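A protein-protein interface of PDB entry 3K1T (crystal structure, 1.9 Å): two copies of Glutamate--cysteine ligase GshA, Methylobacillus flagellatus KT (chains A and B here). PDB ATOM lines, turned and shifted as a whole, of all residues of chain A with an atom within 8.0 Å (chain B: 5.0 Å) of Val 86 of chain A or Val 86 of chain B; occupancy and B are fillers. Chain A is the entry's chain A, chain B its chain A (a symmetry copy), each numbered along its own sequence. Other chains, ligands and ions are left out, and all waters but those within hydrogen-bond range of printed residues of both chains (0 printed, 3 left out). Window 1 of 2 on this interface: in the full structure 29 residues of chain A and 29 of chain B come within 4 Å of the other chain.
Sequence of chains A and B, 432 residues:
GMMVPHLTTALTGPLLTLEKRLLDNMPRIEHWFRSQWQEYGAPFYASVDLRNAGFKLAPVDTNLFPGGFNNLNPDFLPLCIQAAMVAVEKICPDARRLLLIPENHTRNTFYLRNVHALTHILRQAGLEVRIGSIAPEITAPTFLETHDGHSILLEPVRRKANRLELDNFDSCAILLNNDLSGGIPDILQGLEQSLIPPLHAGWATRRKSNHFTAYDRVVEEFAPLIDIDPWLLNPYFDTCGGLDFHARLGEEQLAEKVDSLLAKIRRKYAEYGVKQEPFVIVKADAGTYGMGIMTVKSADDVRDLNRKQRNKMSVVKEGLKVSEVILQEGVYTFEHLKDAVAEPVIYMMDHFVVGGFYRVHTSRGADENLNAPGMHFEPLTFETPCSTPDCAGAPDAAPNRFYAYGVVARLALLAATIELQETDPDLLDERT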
ATOM      1  N   ARG A  34     -34.106  28.536 -28.146  1.00  0.00           N
ATOM      2  CA  ARG A  34     -33.003  28.275 -29.085  1.00  0.00           C
ATOM      3  C   ARG A  34     -33.205  28.974 -30.430  1.00  0.00           C
ATOM      4  O   ARG A  34     -32.229  29.544 -30.954  1.00  0.00           O
ATOM      5  CB  ARG A  34     -32.742  26.780 -29.293  1.00  0.00           C
ATOM      6  CG  ARG A  34     -31.927  26.195 -28.138  1.00  0.00           C
ATOM      7  CD  ARG A  34     -31.523  24.753 -28.449  1.00  0.00           C
ATOM      8  NE  ARG A  34     -32.572  23.777 -28.264  1.00  0.00           N
ATOM      9  CZ  ARG A  34     -32.767  23.124 -27.107  1.00  0.00           C
ATOM     10  NH1 ARG A  34     -32.001  23.357 -26.039  1.00  0.00           N
ATOM     11  NH2 ARG A  34     -33.723  22.256 -27.036  1.00  0.00           N
ATOM     12  N   PHE A  44     -23.038  39.123 -23.086  1.00  0.00           N
ATOM     13  CA  PHE A  44     -21.986  38.385 -22.380  1.00  0.00           C
ATOM     14  C   PHE A  44     -22.487  37.943 -20.992  1.00  0.00           C
ATOM     15  O   PHE A  44     -22.284  36.797 -20.572  1.00  0.00           O
ATOM     16  CB  PHE A  44     -20.708  39.277 -22.256  1.00  0.00           C
ATOM     17  CG  PHE A  44     -19.522  38.553 -21.704  1.00  0.00           C
ATOM     18  CD1 PHE A  44     -18.643  37.894 -22.554  1.00  0.00           C
ATOM     19  CD2 PHE A  44     -19.278  38.523 -20.336  1.00  0.00           C
ATOM     20  CE1 PHE A  44     -17.574  37.180 -22.069  1.00  0.00           C
ATOM     21  CE2 PHE A  44     -18.188  37.821 -19.833  1.00  0.00           C
ATOM     22  CZ  PHE A  44     -17.334  37.143 -20.706  1.00  0.00           C
ATOM     23  N   LEU A  79     -20.478  25.779 -13.092  1.00  0.00           N
ATOM     24  CA  LEU A  79     -21.535  26.135 -14.042  1.00  0.00           C
ATOM     25  C   LEU A  79     -21.301  27.551 -14.597  1.00  0.00           C
ATOM     26  O   LEU A  79     -21.452  27.806 -15.792  1.00  0.00           O
ATOM     27  CB  LEU A  79     -22.887  26.060 -13.352  1.00  0.00           C
ATOM     28  CG  LEU A  79     -24.136  26.324 -14.197  1.00  0.00           C
ATOM     29  CD1 LEU A  79     -24.339  25.094 -15.032  1.00  0.00           C
ATOM     30  CD2 LEU A  79     -25.379  26.531 -13.294  1.00  0.00           C
ATOM     31  N   CYS A  80     -20.908  28.476 -13.728  1.00  0.00           N
ATOM     32  CA  CYS A  80     -20.556  29.838 -14.168  1.00  0.00           C
ATOM     33  C   CYS A  80     -19.386  29.880 -15.088  1.00  0.00           C
ATOM     34  O   CYS A  80     -19.381  30.623 -16.096  1.00  0.00           O
ATOM     35  CB  CYS A  80     -20.200  30.749 -12.990  1.00  0.00           C
ATOM     36  SG  CYS A  80     -21.530  31.194 -11.995  1.00  0.00           S
ATOM     37  N   ILE A  81     -18.352  29.134 -14.757  1.00  0.00           N
ATOM     38  CA  ILE A  81     -17.145  29.066 -15.569  1.00  0.00           C
ATOM     39  C   ILE A  81     -17.461  28.546 -16.979  1.00  0.00           C
ATOM     40  O   ILE A  81     -16.999  29.111 -18.004  1.00  0.00           O
ATOM     41  CB  ILE A  81     -16.019  28.235 -14.886  1.00  0.00           C
ATOM     42  CG1 ILE A  81     -15.595  28.929 -13.590  1.00  0.00           C
ATOM     43  CG2 ILE A  81     -14.829  27.937 -15.882  1.00  0.00           C
ATOM     44  CD1 ILE A  81     -14.784  28.042 -12.603  1.00  0.00           C
ATOM     45  N   GLN A  82     -18.259  27.473 -17.043  1.00  0.00           N
ATOM     46  CA  GLN A  82     -18.608  26.901 -18.325  1.00  0.00           C
ATOM     47  C   GLN A  82     -19.412  27.901 -19.178  1.00  0.00           C
ATOM     48  O   GLN A  82     -19.139  28.094 -20.372  1.00  0.00           O
ATOM     49  CB  GLN A  82     -19.403  25.604 -18.119  1.00  0.00           C
ATOM     50  CG  GLN A  82     -19.661  24.835 -19.397  1.00  0.00           C
ATOM     51  CD  GLN A  82     -20.453  23.567 -19.107  1.00  0.00           C
ATOM     52  OE1 GLN A  82     -19.878  22.528 -18.786  1.00  0.00           O
ATOM     53  NE2 GLN A  82     -21.739  23.656 -19.222  1.00  0.00           N
ATOM     54  N   ALA A  83     -20.378  28.575 -18.548  1.00  0.00           N
ATOM     55  CA  ALA A  83     -21.182  29.558 -19.265  1.00  0.00           C
ATOM     56  C   ALA A  83     -20.309  30.736 -19.723  1.00  0.00           C
ATOM     57  O   ALA A  83     -20.491  31.278 -20.794  1.00  0.00           O
ATOM     58  CB  ALA A  83     -22.354  30.036 -18.367  1.00  0.00           C
ATOM     59  N   ALA A  84     -19.375  31.160 -18.883  1.00  0.00           N
ATOM     60  CA  ALA A  84     -18.459  32.238 -19.257  1.00  0.00           C
ATOM     61  C   ALA A  84     -17.605  31.796 -20.452  1.00  0.00           C
ATOM     62  O   ALA A  84     -17.373  32.575 -21.365  1.00  0.00           O
ATOM     63  CB  ALA A  84     -17.542  32.617 -18.084  1.00  0.00           C
ATOM     64  N   MET A  85     -17.163  30.545 -20.472  1.00  0.00           N
ATOM     65  CA  MET A  85     -16.449  30.033 -21.661  1.00  0.00           C
ATOM     66  C   MET A  85     -17.264  30.057 -22.948  1.00  0.00           C
ATOM     67  O   MET A  85     -16.760  30.442 -24.005  1.00  0.00           O
ATOM     68  CB  MET A  85     -15.907  28.612 -21.447  1.00  0.00           C
ATOM     69  CG  MET A  85     -14.745  28.610 -20.532  1.00  0.00           C
ATOM     70  SD  MET A  85     -14.187  26.751 -20.165  1.00  0.00           S
ATOM     71  CE  MET A  85     -12.271  27.145 -19.830  1.00  0.00           C
ATOM     72  N   VAL A  86     -18.530  29.686 -22.856  1.00  0.00           N
ATOM     73  CA  VAL A  86     -19.456  29.820 -24.001  1.00  0.00           C
ATOM     74  C   VAL A  86     -19.546  31.279 -24.453  1.00  0.00           C
ATOM     75  O   VAL A  86     -19.448  31.570 -25.634  1.00  0.00           O
ATOM     76  CB  VAL A  86     -20.864  29.271 -23.629  1.00  0.00           C
ATOM     77  CG1 VAL A  86     -21.896  29.551 -24.757  1.00  0.00           C
ATOM     78  CG2 VAL A  86     -20.772  27.751 -23.345  1.00  0.00           C
ATOM     79  N   ALA A  87     -19.743  32.204 -23.508  1.00  0.00           N
ATOM     80  CA  ALA A  87     -19.806  33.638 -23.817  1.00  0.00           C
ATOM     81  C   ALA A  87     -18.534  34.111 -24.531  1.00  0.00           C
ATOM     82  O   ALA A  87     -18.613  34.787 -25.555  1.00  0.00           O
ATOM     83  CB  ALA A  87     -20.040  34.481 -22.539  1.00  0.00           C
ATOM     84  N   VAL A  88     -17.369  33.758 -24.002  1.00  0.00           N
ATOM     85  CA  VAL A  88     -16.105  34.062 -24.675  1.00  0.00           C
ATOM     86  C   VAL A  88     -16.066  33.531 -26.116  1.00  0.00           C
ATOM     87  O   VAL A  88     -15.663  34.255 -27.040  1.00  0.00           O
ATOM     88  CB  VAL A  88     -14.922  33.537 -23.871  1.00  0.00           C
ATOM     89  CG1 VAL A  88     -13.584  33.571 -24.712  1.00  0.00           C
ATOM     90  CG2 VAL A  88     -14.814  34.302 -22.538  1.00  0.00           C
ATOM     91  N   GLU A  89     -16.452  32.277 -26.320  1.00  0.00           N
ATOM     92  CA  GLU A  89     -16.454  31.685 -27.652  1.00  0.00           C
ATOM     93  C   GLU A  89     -17.412  32.349 -28.640  1.00  0.00           C
ATOM     94  O   GLU A  89     -17.146  32.322 -29.833  1.00  0.00           O
ATOM     95  CB  GLU A  89     -16.801  30.195 -27.591  1.00  0.00           C
ATOM     96  CG  GLU A  89     -15.754  29.354 -26.917  1.00  0.00           C
ATOM     97  CD  GLU A  89     -16.234  27.923 -26.646  1.00  0.00           C
ATOM     98  OE1 GLU A  89     -17.169  27.479 -27.358  1.00  0.00           O
ATOM     99  OE2 GLU A  89     -15.677  27.274 -25.728  1.00  0.00           O
ATOM    100  N   LYS A  90     -18.521  32.935 -28.167  1.00  0.00           N
ATOM    101  CA  LYS A  90     -19.497  33.593 -29.044  1.00  0.00           C
ATOM    102  C   LYS A  90     -19.159  35.059 -29.276  1.00  0.00           C
ATOM    103  O   LYS A  90     -19.357  35.565 -30.380  1.00  0.00           O
ATOM    104  CB  LYS A  90     -20.919  33.535 -28.455  1.00  0.00           C
ATOM    105  CG  LYS A  90     -21.508  32.147 -28.560  1.00  0.00           C
ATOM    106  CD  LYS A  90     -22.892  32.051 -28.009  1.00  0.00           C
ATOM    107  CE  LYS A  90     -23.323  30.594 -28.061  1.00  0.00           C
ATOM    108  NZ  LYS A  90     -24.564  30.385 -27.340  1.00  0.00           N
ATOM    109  N   ILE A  91     -18.659  35.727 -28.251  1.00  0.00           N
ATOM    110  CA  ILE A  91     -18.529  37.191 -28.271  1.00  0.00           C
ATOM    111  C   ILE A  91     -17.099  37.662 -28.525  1.00  0.00           C
ATOM    112  O   ILE A  91     -16.895  38.711 -29.125  1.00  0.00           O
ATOM    113  CB  ILE A  91     -19.015  37.813 -26.940  1.00  0.00           C
ATOM    114  CG1 ILE A  91     -20.503  37.488 -26.679  1.00  0.00           C
ATOM    115  CG2 ILE A  91     -18.776  39.333 -26.916  1.00  0.00           C
ATOM    116  CD1 ILE A  91     -21.463  37.956 -27.800  1.00  0.00           C
ATOM    117  N   CYS A  92     -16.110  36.930 -28.029  1.00  0.00           N
ATOM    118  CA  CYS A  92     -14.711  37.307 -28.310  1.00  0.00           C
ATOM    119  C   CYS A  92     -13.841  36.045 -28.501  1.00  0.00           C
ATOM    120  O   CYS A  92     -12.947  35.750 -27.700  1.00  0.00           O
ATOM    121  CB  CYS A  92     -14.173  38.256 -27.218  1.00  0.00           C
ATOM    122  SG  CYS A  92     -14.376  37.710 -25.529  1.00  0.00           S
ATOM    123  N   PRO A  93     -14.101  35.300 -29.594  1.00  0.00           N
ATOM    124  CA  PRO A  93     -13.603  33.929 -29.695  1.00  0.00           C
ATOM    125  C   PRO A  93     -12.109  33.765 -29.658  1.00  0.00           C
ATOM    126  O   PRO A  93     -11.633  32.709 -29.231  1.00  0.00           O
ATOM    127  CB  PRO A  93     -14.168  33.431 -31.049  1.00  0.00           C
ATOM    128  CG  PRO A  93     -14.647  34.625 -31.763  1.00  0.00           C
ATOM    129  CD  PRO A  93     -15.037  35.615 -30.682  1.00  0.00           C
ATOM    130  N   ALA A 125     -12.107  30.841 -16.838  1.00  0.00           N
ATOM    131  CA  ALA A 125     -12.513  30.650 -18.223  1.00  0.00           C
ATOM    132  C   ALA A 125     -11.346  30.709 -19.186  1.00  0.00           C
ATOM    133  O   ALA A 125     -11.519  30.488 -20.376  1.00  0.00           O
ATOM    134  CB  ALA A 125     -13.660  31.671 -18.627  1.00  0.00           C
ATOM    135  N   MET A 349     -25.098  34.182 -17.985  1.00  0.00           N
ATOM    136  CA  MET A 349     -23.945  34.418 -18.856  1.00  0.00           C
ATOM    137  C   MET A 349     -24.232  33.751 -20.191  1.00  0.00           C
ATOM    138  O   MET A 349     -24.780  32.630 -20.237  1.00  0.00           O
ATOM    139  CB  MET A 349     -22.656  33.913 -18.192  1.00  0.00           C
ATOM    140  CG  MET A 349     -22.442  34.582 -16.854  1.00  0.00           C
ATOM    141  SD  MET A 349     -20.639  34.215 -16.122  1.00  0.00           S
ATOM    142  CE  MET A 349     -19.767  35.603 -17.146  1.00  0.00           C
ATOM    143  N   ASP A 350     -23.962  34.457 -21.281  1.00  0.00           N
ATOM    144  CA  ASP A 350     -24.534  34.085 -22.588  1.00  0.00           C
ATOM    145  C   ASP A 350     -26.046  33.905 -22.337  1.00  0.00           C
ATOM    146  O   ASP A 350     -26.634  34.686 -21.561  1.00  0.00           O
ATOM    147  CB  ASP A 350     -23.851  32.847 -23.212  1.00  0.00           C
ATOM    148  CG  ASP A 350     -24.322  32.578 -24.647  1.00  0.00           C
ATOM    149  OD1 ASP A 350     -24.263  33.491 -25.446  1.00  0.00           O
ATOM    150  OD2 ASP A 350     -24.785  31.486 -24.966  1.00  0.00           O
ATOM    151  N   HIS A 351     -26.698  32.890 -22.910  1.00  0.00           N
ATOM    152  CA  HIS A 351     -28.153  32.752 -22.662  1.00  0.00           C
ATOM    153  C   HIS A 351     -28.472  31.693 -21.593  1.00  0.00           C
ATOM    154  O   HIS A 351     -29.572  31.136 -21.586  1.00  0.00           O
ATOM    155  CB  HIS A 351     -28.910  32.482 -23.963  1.00  0.00           C
ATOM    156  CG  HIS A 351     -28.415  31.290 -24.748  1.00  0.00           C
ATOM    157  ND1 HIS A 351     -27.761  31.418 -25.963  1.00  0.00           N
ATOM    158  CD2 HIS A 351     -28.488  29.958 -24.495  1.00  0.00           C
ATOM    159  CE1 HIS A 351     -27.472  30.209 -26.424  1.00  0.00           C
ATOM    160  NE2 HIS A 351     -27.907  29.307 -25.559  1.00  0.00           N
ATOM    161  N   PHE A 352     -27.530  31.412 -20.697  1.00  0.00           N
ATOM    162  CA  PHE A 352     -27.689  30.370 -19.676  1.00  0.00           C
ATOM    163  C   PHE A 352     -27.876  30.982 -18.299  1.00  0.00           C
ATOM    164  O   PHE A 352     -27.137  31.903 -17.900  1.00  0.00           O
ATOM    165  CB  PHE A 352     -26.479  29.437 -19.672  1.00  0.00           C
ATOM    166  CG  PHE A 352     -26.353  28.652 -20.934  1.00  0.00           C
ATOM    167  CD1 PHE A 352     -27.336  27.708 -21.267  1.00  0.00           C
ATOM    168  CD2 PHE A 352     -25.344  28.877 -21.798  1.00  0.00           C
ATOM    169  CE1 PHE A 352     -27.238  26.978 -22.450  1.00  0.00           C
ATOM    170  CE2 PHE A 352     -25.266  28.169 -23.014  1.00  0.00           C
ATOM    171  CZ  PHE A 352     -26.229  27.239 -23.332  1.00  0.00           C
ATOM    172  N   GLN B  82     -26.398  21.987 -19.029  1.00  0.00           N
ATOM    173  CA  GLN B  82     -25.941  23.137 -19.780  1.00  0.00           C
ATOM    174  C   GLN B  82     -25.031  22.709 -20.947  1.00  0.00           C
ATOM    175  O   GLN B  82     -25.181  23.178 -22.085  1.00  0.00           O
ATOM    176  CB  GLN B  82     -25.207  24.110 -18.849  1.00  0.00           C
ATOM    177  CG  GLN B  82     -24.847  25.427 -19.502  1.00  0.00           C
ATOM    178  CD  GLN B  82     -24.123  26.334 -18.516  1.00  0.00           C
ATOM    179  OE1 GLN B  82     -24.754  27.065 -17.756  1.00  0.00           O
ATOM    180  NE2 GLN B  82     -22.829  26.282 -18.534  1.00  0.00           N
ATOM    181  N   ALA B  83     -24.112  21.779 -20.674  1.00  0.00           N
ATOM    182  CA  ALA B  83     -23.216  21.296 -21.717  1.00  0.00           C
ATOM    183  C   ALA B  83     -24.007  20.556 -22.806  1.00  0.00           C
ATOM    184  O   ALA B  83     -23.707  20.651 -23.979  1.00  0.00           O
ATOM    185  CB  ALA B  83     -22.124  20.386 -21.093  1.00  0.00           C
ATOM    186  N   ALA B  84     -25.007  19.781 -22.408  1.00  0.00           N
ATOM    187  CA  ALA B  84     -25.852  19.085 -23.379  1.00  0.00           C
ATOM    188  C   ALA B  84     -26.597  20.111 -24.242  1.00  0.00           C
ATOM    189  O   ALA B  84     -26.717  19.932 -25.445  1.00  0.00           O
ATOM    190  CB  ALA B  84     -26.868  18.173 -22.675  1.00  0.00           C
ATOM    191  N   MET B  85     -27.070  21.198 -23.647  1.00  0.00           N
ATOM    192  CA  MET B  85     -27.678  22.277 -24.454  1.00  0.00           C
ATOM    193  C   MET B  85     -26.741  22.907 -25.476  1.00  0.00           C
ATOM    194  O   MET B  85     -27.130  23.147 -26.622  1.00  0.00           O
ATOM    195  CB  MET B  85     -28.278  23.390 -23.582  1.00  0.00           C
ATOM    196  CG  MET B  85     -29.522  22.944 -22.919  1.00  0.00           C
ATOM    197  SD  MET B  85     -30.164  24.350 -21.689  1.00  0.00           S
ATOM    198  CE  MET B  85     -32.093  23.892 -21.799  1.00  0.00           C
ATOM    199  N   VAL B  86     -25.501  23.141 -25.080  1.00  0.00           N
ATOM    200  CA  VAL B  86     -24.465  23.601 -26.030  1.00  0.00           C
ATOM    201  C   VAL B  86     -24.291  22.593 -27.167  1.00  0.00           C
ATOM    202  O   VAL B  86     -24.265  22.967 -28.329  1.00  0.00           O
ATOM    203  CB  VAL B  86     -23.115  23.834 -25.291  1.00  0.00           C
ATOM    204  CG1 VAL B  86     -21.970  24.158 -26.292  1.00  0.00           C
ATOM    205  CG2 VAL B  86     -23.277  24.983 -24.263  1.00  0.00           C
ATOM    206  N   ALA B  87     -24.161  21.305 -26.834  1.00  0.00           N
ATOM    207  CA  ALA B  87     -24.029  20.244 -27.840  1.00  0.00           C
ATOM    208  C   ALA B  87     -25.211  20.251 -28.816  1.00  0.00           C
ATOM    209  O   ALA B  87     -25.014  20.209 -30.029  1.00  0.00           O
ATOM    210  CB  ALA B  87     -23.897  18.850 -27.177  1.00  0.00           C
ATOM    211  N   VAL B  88     -26.432  20.306 -28.296  1.00  0.00           N
ATOM    212  CA  VAL B  88     -27.615  20.434 -29.149  1.00  0.00           C
ATOM    213  C   VAL B  88     -27.529  21.643 -30.094  1.00  0.00           C
ATOM    214  O   VAL B  88     -27.819  21.522 -31.294  1.00  0.00           O
ATOM    215  CB  VAL B  88     -28.885  20.493 -28.308  1.00  0.00           C
ATOM    216  CG1 VAL B  88     -30.133  20.942 -29.168  1.00  0.00           C
ATOM    217  CG2 VAL B  88     -29.102  19.147 -27.592  1.00  0.00           C
ATOM    218  N   GLU B  89     -27.160  22.806 -29.572  1.00  0.00           N
ATOM    219  CA  GLU B  89     -27.044  24.008 -30.388  1.00  0.00           C
ATOM    220  C   GLU B  89     -25.976  23.933 -31.479  1.00  0.00           C
ATOM    221  O   GLU B  89     -26.126  24.589 -32.501  1.00  0.00           O
ATOM    222  CB  GLU B  89     -26.746  25.235 -29.523  1.00  0.00           C
ATOM    223  CG  GLU B  89     -27.876  25.627 -28.615  1.00  0.00           C
ATOM    224  CD  GLU B  89     -27.464  26.690 -27.589  1.00  0.00           C
ATOM    225  OE1 GLU B  89     -26.478  27.416 -27.867  1.00  0.00           O
ATOM    226  OE2 GLU B  89     -28.126  26.778 -26.526  1.00  0.00           O
ATOM    227  N   LYS B  90     -24.903  23.156 -31.278  1.00  0.00           N
ATOM    228  CA  LYS B  90     -23.829  23.029 -32.270  1.00  0.00           C
ATOM    229  C   LYS B  90     -24.101  21.912 -33.268  1.00  0.00           C
ATOM    230  O   LYS B  90     -23.783  22.053 -34.447  1.00  0.00           O
ATOM    231  CB  LYS B  90     -22.473  22.730 -31.602  1.00  0.00           C
ATOM    232  CG  LYS B  90     -21.915  23.951 -30.907  1.00  0.00           C
ATOM    233  CD  LYS B  90     -20.594  23.706 -30.255  1.00  0.00           C
ATOM    234  CE  LYS B  90     -20.200  24.961 -29.494  1.00  0.00           C
ATOM    235  NZ  LYS B  90     -19.042  24.727 -28.654  1.00  0.00           N
ATOM    236  N   ILE B  91     -24.681  20.820 -32.798  1.00  0.00           N
ATOM    237  CA  ILE B  91     -24.767  19.587 -33.595  1.00  0.00           C
ATOM    238  C   ILE B  91     -26.152  19.360 -34.196  1.00  0.00           C
ATOM    239  O   ILE B  91     -26.267  18.786 -35.273  1.00  0.00           O
ATOM    240  CB  ILE B  91     -24.396  18.348 -32.747  1.00  0.00           C
ATOM    241  CG1 ILE B  91     -22.950  18.446 -32.211  1.00  0.00           C
ATOM    242  CG2 ILE B  91     -24.594  17.047 -33.546  1.00  0.00           C
ATOM    243  CD1 ILE B  91     -21.873  18.608 -33.311  1.00  0.00           C
ATOM    244  N   ASP B 350     -20.118  18.103 -25.718  1.00  0.00           N
ATOM    245  CA  ASP B 350     -19.433  19.089 -26.574  1.00  0.00           C
ATOM    246  C   ASP B 350     -17.958  19.069 -26.120  1.00  0.00           C
ATOM    247  O   ASP B 350     -17.426  17.981 -25.814  1.00  0.00           O
ATOM    248  CB  ASP B 350     -20.085  20.489 -26.519  1.00  0.00           C
ATOM    249  CG  ASP B 350     -19.484  21.457 -27.547  1.00  0.00           C
ATOM    250  OD1 ASP B 350     -19.440  21.099 -28.708  1.00  0.00           O
ATOM    251  OD2 ASP B 350     -19.023  22.540 -27.200  1.00  0.00           O
ATOM    252  N   PHE B 352     -16.710  20.291 -23.281  1.00  0.00           N
ATOM    253  CA  PHE B 352     -16.680  20.639 -21.856  1.00  0.00           C
ATOM    254  C   PHE B 352     -16.612  19.392 -20.993  1.00  0.00           C
ATOM    255  O   PHE B 352     -17.359  18.419 -21.210  1.00  0.00           O
ATOM    256  CB  PHE B 352     -17.910  21.465 -21.481  1.00  0.00           C
ATOM    257  CG  PHE B 352     -17.934  22.797 -22.151  1.00  0.00           C
ATOM    258  CD1 PHE B 352     -16.950  23.749 -21.842  1.00  0.00           C
ATOM    259  CD2 PHE B 352     -18.848  23.086 -23.098  1.00  0.00           C
ATOM    260  CE1 PHE B 352     -16.952  24.993 -22.471  1.00  0.00           C
ATOM    261  CE2 PHE B 352     -18.826  24.329 -23.764  1.00  0.00           C
ATOM    262  CZ  PHE B 352     -17.863  25.260 -23.451  1.00  0.00           C
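The side-chain carboxylate (OD2) of Asp 350 of chain A sits at hydrogen-bond distance from a ring nitrogen (ND1) of His 351 of chain A (3.1 Å).
NZ of Lys 90 of chain B lies within salt-bridge range of OD2 of Asp 350 of chain B (2.6 Å).
The side-chain amino group (NZ) of Lys 90 of chain A lies within salt-bridge range of the side-chain carboxylate (OD2) of Asp 350 of chain A, 2.6 Å away.
Printed residues of chain B within 4 Å of His 351 of chain A: Glu 89 (2.7 Å).
No residue of chain A comes within 4 Å of Ala 87 of chain B.
Of the printed residues of chain A, Val 88 of chain B touches Arg 34 (3.8 Å).
The nearest printed residue of chain B that does not touch Val 86 of chain A is Gln 82 of chain B (5.4 Å).
NE2 of Gln 82 of chain A sits close to N of Ala 83 of chain B (3.4 Å).
The side-chain carboxylate (OE2) of Glu 89 of chain B sits at hydrogen-bond distance from a ring nitrogen (NE2) of His 351 of chain A (2.7 Å).
The side-chain amino group of Lys 90 of chain A is in salt-bridge range of the side-chain carboxylate of Glu 89 of chain B (3.6 Å).
The side-chain amide nitrogen of Gln 82 of chain A lies close to the side-chain amide nitrogen of Gln 82 of chain B (2.9 Å).
OE1 of Glu 89 of chain A lies within salt-bridge range of NZ of Lys 90 of chain B.
The backbone NH of Ala 83 of chain A lies close to the side-chain amide nitrogen of Gln 82 of chain B (3.4 Å).
The side-chain amide nitrogen of Gln 82 of chain B lies within hydrogen-bond range of the backbone carbonyl oxygen of Leu 79 of chain A.
CG1 of Val 88 of chain B touches NE of Arg 34 of chain A, 3.8 Å away.
CD of Arg 34 of chain A touches CG of Glu 89 of chain B (3.8 Å).
OE1 of Gln 82 of chain A touches CB of Phe 352 of chain B (3.5 Å).
Met 85 of chain A touches Phe 352 of chain B (CB to CE1, 3.9 Å).
Val 86 of chain B touches Val 86 of chain A (CG2 to CG2, 3.8 Å).
Glu 89 of chain A touches Phe 352 of chain B.
OE1 of Gln 82 of chain B touches CB of Phe 352 of chain A, 3.5 Å away.
Met 85 of chain B touches Phe 352 of chain A (CB to CE1, 3.9 Å).
Val 86 of chain B touches Phe 352 of chain A.
Glu 89 of chain B touches Phe 352 of chain A (OE2 to CZ, 3.7 Å).
Of the 12 printed residues of chain B, 8 touch a printed residue of chain A.
Of the 22 printed residues of chain A, 10 touch a printed residue of chain B.
Printed residues of chain A that touch a printed residue of chain B: Arg 34, Leu 79, Gln 82, Ala 83, Met 85, Val 86, Glu 89, Lys 90, His 351 and Phe 352.
Among the printed residues, Asp or Glu carboxylates within 4 Å of a Lys or Arg side-chain nitrogen of the other chain: Glu 89 of chain A with Lys 90 of chain B (3.6 Å) and Lys 90 of chain A with Glu 89 of chain B (3.6 Å).
Gln 82 of chain A touches Phe 352 of chain B, and with the chains exchanged Phe 352 of chain A touches Gln 82 of chain B.
Val 86 of chain A touches Phe 352 of chain B, and with the chains exchanged Phe 352 of chain A touches Val 86 of chain B.
Glu 89 of chain A touches Lys 90 of chain B, and with the chains exchanged Lys 90 of chain A touches Glu 89 of chain B.
Glu 89 of chain A touches Phe 352 of chain B, and with the chains exchanged Phe 352 of chain A touches Glu 89 of chain B.
Positions printed for both chains: 82, 83, 84, 85, 86, 87, 88, 89, 90, 91, 350 and 352.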
